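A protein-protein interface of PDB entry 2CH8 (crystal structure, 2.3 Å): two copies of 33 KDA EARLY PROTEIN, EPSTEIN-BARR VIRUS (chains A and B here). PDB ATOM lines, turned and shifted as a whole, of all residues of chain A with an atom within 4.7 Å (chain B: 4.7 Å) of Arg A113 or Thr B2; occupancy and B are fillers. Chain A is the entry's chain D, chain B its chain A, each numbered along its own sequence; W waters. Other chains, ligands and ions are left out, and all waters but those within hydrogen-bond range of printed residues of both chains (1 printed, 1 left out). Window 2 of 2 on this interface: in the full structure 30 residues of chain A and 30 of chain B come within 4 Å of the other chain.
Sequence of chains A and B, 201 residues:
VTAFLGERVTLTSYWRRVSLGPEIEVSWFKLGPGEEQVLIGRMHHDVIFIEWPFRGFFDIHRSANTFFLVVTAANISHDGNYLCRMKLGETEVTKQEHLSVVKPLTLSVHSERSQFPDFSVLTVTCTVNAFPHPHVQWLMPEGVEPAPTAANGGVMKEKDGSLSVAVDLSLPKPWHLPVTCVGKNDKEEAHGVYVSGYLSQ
OE2 of Glu B7 lies within salt-bridge range of NE of Arg A113 (2.9 Å).
The backbone NH (N) of Phe B4 is in hydrogen-bond range of the side-chain carboxylate (OE1) of Glu B7, at 2.9 Å.
Arg A113 touches Thr B2.
NE of Arg A113 touches CD1 of Phe B4, at 3.4 Å.
Gln A115 touches Glu B7.
Leu A199 touches Phe B4.
Of chain B, only Thr B2, Phe B4 and Glu B7 come within 4 Å of Arg A113.
Of the printed residues of chain A, Thr B2 touches Arg A113.
Printed residues of chain A within 4 Å of Phe B4: Arg A113 and Leu A199.
Of the printed residues of chain B, Leu A199 touches Phe B4 (3.3 Å).
The nearest printed residue of chain A that does not touch Thr B2 is Leu A199 (4.01 Å).
Of the 9 printed residues of chain A, 3 touch a printed residue of chain B.
Hydrophobic or aromatic side chains of chain A within 4 Å of the printed part of chain B: Leu A199.
Of the 7 printed residues of chain B, 3 touch a printed residue of chain A.
Along chain B the printed residues that touch a printed residue of chain A span positions 2 to 7.
Among the printed residues, Asp or Glu carboxylates within 4 Å of a Lys or Arg side-chain nitrogen of the other chain: Arg A113 with Glu B7 (2.9 Å).
No position is printed for both chains.
Water W1 bridges O of Thr B2 and NH2 of Arg A113.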
ATOM      1  N   SER A 111     -11.151  11.724 -17.525  1.00  0.00           N
ATOM      2  CA  SER A 111     -12.281  11.348 -18.341  1.00  0.00           C
ATOM      3  C   SER A 111     -13.552  11.731 -17.634  1.00  0.00           C
ATOM      4  O   SER A 111     -13.547  11.935 -16.422  1.00  0.00           O
ATOM      5  CB  SER A 111     -12.275   9.865 -18.693  1.00  0.00           C
ATOM      6  OG  SER A 111     -12.855   9.158 -17.636  1.00  0.00           O
ATOM      7  N   GLU A 112     -14.631  11.844 -18.401  1.00  0.00           N
ATOM      8  CA  GLU A 112     -15.897  12.219 -17.870  1.00  0.00           C
ATOM      9  C   GLU A 112     -16.971  11.643 -18.770  1.00  0.00           C
ATOM     10  O   GLU A 112     -16.987  11.949 -19.952  1.00  0.00           O
ATOM     11  CB  GLU A 112     -15.968  13.732 -17.921  1.00  0.00           C
ATOM     12  CG  GLU A 112     -17.118  14.299 -17.162  1.00  0.00           C
ATOM     13  CD  GLU A 112     -17.178  15.800 -17.286  1.00  0.00           C
ATOM     14  OE1 GLU A 112     -16.154  16.456 -16.946  1.00  0.00           O
ATOM     15  OE2 GLU A 112     -18.251  16.304 -17.704  1.00  0.00           O
ATOM     16  N   ARG A 113     -17.878  10.828 -18.227  1.00  0.00           N
ATOM     17  CA  ARG A 113     -19.045  10.358 -18.980  1.00  0.00           C
ATOM     18  C   ARG A 113     -20.090  11.458 -19.230  1.00  0.00           C
ATOM     19  O   ARG A 113     -20.202  12.438 -18.501  1.00  0.00           O
ATOM     20  CB  ARG A 113     -19.685   9.151 -18.289  1.00  0.00           C
ATOM     21  CG  ARG A 113     -20.313   9.455 -16.958  1.00  0.00           C
ATOM     22  CD  ARG A 113     -21.010   8.250 -16.482  1.00  0.00           C
ATOM     23  NE  ARG A 113     -21.927   8.523 -15.380  1.00  0.00           N
ATOM     24  CZ  ARG A 113     -22.663   7.582 -14.774  1.00  0.00           C
ATOM     25  NH1 ARG A 113     -22.577   6.326 -15.174  1.00  0.00           N
ATOM     26  NH2 ARG A 113     -23.502   7.893 -13.780  1.00  0.00           N
ATOM     27  N   SER A 114     -20.852  11.301 -20.293  1.00  0.00           N
ATOM     28  CA  SER A 114     -21.904  12.253 -20.609  1.00  0.00           C
ATOM     29  C   SER A 114     -23.027  12.231 -19.540  1.00  0.00           C
ATOM     30  O   SER A 114     -23.193  11.264 -18.813  1.00  0.00           O
ATOM     31  CB  SER A 114     -22.472  11.974 -22.012  1.00  0.00           C
ATOM     32  OG  SER A 114     -22.908  10.638 -22.132  1.00  0.00           O
ATOM     33  N   GLN A 115     -23.757  13.329 -19.462  1.00  0.00           N
ATOM     34  CA  GLN A 115     -24.876  13.488 -18.553  1.00  0.00           C
ATOM     35  C   GLN A 115     -26.245  13.680 -19.271  1.00  0.00           C
ATOM     36  O   GLN A 115     -27.349  13.635 -18.643  1.00  0.00           O
ATOM     37  CB  GLN A 115     -24.569  14.688 -17.661  1.00  0.00           C
ATOM     38  CG  GLN A 115     -23.511  14.295 -16.626  1.00  0.00           C
ATOM     39  CD  GLN A 115     -23.020  15.432 -15.807  1.00  0.00           C
ATOM     40  OE1 GLN A 115     -21.798  15.602 -15.648  1.00  0.00           O
ATOM     41  NE2 GLN A 115     -23.941  16.231 -15.280  1.00  0.00           N
ATOM     42  N   PHE A 119     -25.692   8.462 -20.342  1.00  0.00           N
ATOM     43  CA  PHE A 119     -24.401   8.382 -19.662  1.00  0.00           C
ATOM     44  C   PHE A 119     -23.424   7.459 -20.347  1.00  0.00           C
ATOM     45  O   PHE A 119     -22.471   6.976 -19.718  1.00  0.00           O
ATOM     46  CB  PHE A 119     -24.589   7.877 -18.232  1.00  0.00           C
ATOM     47  CG  PHE A 119     -25.605   8.652 -17.458  1.00  0.00           C
ATOM     48  CD1 PHE A 119     -25.225   9.774 -16.701  1.00  0.00           C
ATOM     49  CD2 PHE A 119     -26.945   8.268 -17.477  1.00  0.00           C
ATOM     50  CE1 PHE A 119     -26.191  10.523 -15.977  1.00  0.00           C
ATOM     51  CE2 PHE A 119     -27.899   9.003 -16.752  1.00  0.00           C
ATOM     52  CZ  PHE A 119     -27.502  10.130 -16.012  1.00  0.00           C
ATOM     53  N   VAL A 121     -21.545   8.010 -23.189  1.00  0.00           N
ATOM     54  CA  VAL A 121     -20.377   8.568 -23.918  1.00  0.00           C
ATOM     55  C   VAL A 121     -19.193   8.949 -22.999  1.00  0.00           C
ATOM     56  O   VAL A 121     -19.312   9.776 -22.119  1.00  0.00           O
ATOM     57  CB  VAL A 121     -20.751   9.736 -24.893  1.00  0.00           C
ATOM     58  CG1 VAL A 121     -19.523  10.261 -25.594  1.00  0.00           C
ATOM     59  CG2 VAL A 121     -21.783   9.275 -25.943  1.00  0.00           C
ATOM     60  N   LEU A 122     -18.035   8.341 -23.225  1.00  0.00           N
ATOM     61  CA  LEU A 122     -16.819   8.700 -22.440  1.00  0.00           C
ATOM     62  C   LEU A 122     -16.069   9.791 -23.192  1.00  0.00           C
ATOM     63  O   LEU A 122     -15.680   9.578 -24.336  1.00  0.00           O
ATOM     64  CB  LEU A 122     -15.962   7.454 -22.214  1.00  0.00           C
ATOM     65  CG  LEU A 122     -15.036   7.281 -21.002  1.00  0.00           C
ATOM     66  CD1 LEU A 122     -13.656   7.697 -21.376  1.00  0.00           C
ATOM     67  CD2 LEU A 122     -15.519   7.993 -19.734  1.00  0.00           C
ATOM     68  N   LEU A 199     -16.432   2.399 -13.865  1.00  0.00           N
ATOM     69  CA  LEU A 199     -17.455   1.373 -14.028  1.00  0.00           C
ATOM     70  C   LEU A 199     -17.286   0.632 -15.360  1.00  0.00           C
ATOM     71  O   LEU A 199     -16.783   1.233 -16.354  1.00  0.00           O
ATOM     72  CB  LEU A 199     -18.838   2.014 -13.983  1.00  0.00           C
ATOM     73  CG  LEU A 199     -19.588   2.372 -12.680  1.00  0.00           C
ATOM     74  CD1 LEU A 199     -19.017   1.948 -11.281  1.00  0.00           C
ATOM     75  CD2 LEU A 199     -19.961   3.831 -12.682  1.00  0.00           C
ATOM     76  N   VAL B   1     -26.570   3.628  -5.417  1.00  0.00           N
ATOM     77  CA  VAL B   1     -26.285   4.173  -6.764  1.00  0.00           C
ATOM     78  C   VAL B   1     -24.920   4.920  -6.752  1.00  0.00           C
ATOM     79  O   VAL B   1     -24.420   5.337  -5.707  1.00  0.00           O
ATOM     80  CB  VAL B   1     -27.526   4.955  -7.417  1.00  0.00           C
ATOM     81  CG1 VAL B   1     -28.910   4.719  -6.634  1.00  0.00           C
ATOM     82  CG2 VAL B   1     -27.269   6.416  -7.675  1.00  0.00           C
ATOM     83  N   THR B   2     -24.309   5.000  -7.934  1.00  0.00           N
ATOM     84  CA  THR B   2     -23.038   5.677  -8.156  1.00  0.00           C
ATOM     85  C   THR B   2     -23.274   6.921  -9.004  1.00  0.00           C
ATOM     86  O   THR B   2     -23.970   6.870 -10.019  1.00  0.00           O
ATOM     87  CB  THR B   2     -22.004   4.739  -8.824  1.00  0.00           C
ATOM     88  OG1 THR B   2     -21.781   3.621  -7.964  1.00  0.00           O
ATOM     89  CG2 THR B   2     -20.670   5.433  -9.080  1.00  0.00           C
ATOM     90  N   ALA B   3     -22.663   8.017  -8.574  1.00  0.00           N
ATOM     91  CA  ALA B   3     -22.781   9.347  -9.181  1.00  0.00           C
ATOM     92  C   ALA B   3     -21.328   9.870  -9.288  1.00  0.00           C
ATOM     93  O   ALA B   3     -20.533   9.740  -8.337  1.00  0.00           O
ATOM     94  CB  ALA B   3     -23.619  10.283  -8.248  1.00  0.00           C
ATOM     95  N   PHE B   4     -20.966  10.439 -10.434  1.00  0.00           N
ATOM     96  CA  PHE B   4     -19.708  11.169 -10.489  1.00  0.00           C
ATOM     97  C   PHE B   4     -19.908  12.596  -9.988  1.00  0.00           C
ATOM     98  O   PHE B   4     -21.036  13.079  -9.960  1.00  0.00           O
ATOM     99  CB  PHE B   4     -19.009  11.000 -11.841  1.00  0.00           C
ATOM    100  CG  PHE B   4     -18.776   9.534 -12.183  1.00  0.00           C
ATOM    101  CD1 PHE B   4     -19.790   8.772 -12.763  1.00  0.00           C
ATOM    102  CD2 PHE B   4     -17.577   8.896 -11.835  1.00  0.00           C
ATOM    103  CE1 PHE B   4     -19.616   7.387 -13.025  1.00  0.00           C
ATOM    104  CE2 PHE B   4     -17.393   7.559 -12.096  1.00  0.00           C
ATOM    105  CZ  PHE B   4     -18.445   6.782 -12.713  1.00  0.00           C
ATOM    106  N   GLU B   7     -22.650  15.416 -10.947  1.00  0.00           N
ATOM    107  CA  GLU B   7     -23.833  14.855 -11.631  1.00  0.00           C
ATOM    108  C   GLU B   7     -25.117  14.996 -10.810  1.00  0.00           C
ATOM    109  O   GLU B   7     -25.101  14.886  -9.590  1.00  0.00           O
ATOM    110  CB  GLU B   7     -23.638  13.372 -11.944  1.00  0.00           C
ATOM    111  CG  GLU B   7     -22.564  13.064 -12.943  1.00  0.00           C
ATOM    112  CD  GLU B   7     -22.493  11.551 -13.333  1.00  0.00           C
ATOM    113  OE1 GLU B   7     -22.903  10.694 -12.520  1.00  0.00           O
ATOM    114  OE2 GLU B   7     -21.999  11.228 -14.434  1.00  0.00           O
ATOM    115  N   SER B 100     -22.742   6.127  -3.803  1.00  0.00           N
ATOM    116  CA  SER B 100     -21.271   6.292  -4.008  1.00  0.00           C
ATOM    117  C   SER B 100     -20.959   7.481  -4.917  1.00  0.00           C
ATOM    118  O   SER B 100     -21.401   7.510  -6.043  1.00  0.00           O
ATOM    119  CB  SER B 100     -20.617   5.042  -4.578  1.00  0.00           C
ATOM    120  OG  SER B 100     -21.031   3.926  -3.835  1.00  0.00           O
ATOM    121  N   VAL B 102     -17.992   9.506  -6.797  1.00  0.00           N
ATOM    122  CA  VAL B 102     -16.693   9.200  -7.348  1.00  0.00           C
ATOM    123  C   VAL B 102     -16.260  10.476  -8.096  1.00  0.00           C
ATOM    124  O   VAL B 102     -17.048  11.080  -8.836  1.00  0.00           O
ATOM    125  CB  VAL B 102     -16.776   8.020  -8.350  1.00  0.00           C
ATOM    126  CG1 VAL B 102     -15.388   7.721  -9.009  1.00  0.00           C
ATOM    127  CG2 VAL B 102     -17.334   6.818  -7.677  1.00  0.00           C
HETATM  128  O   HOH W   1     -24.329   5.203 -12.478  1.00  0.00           O
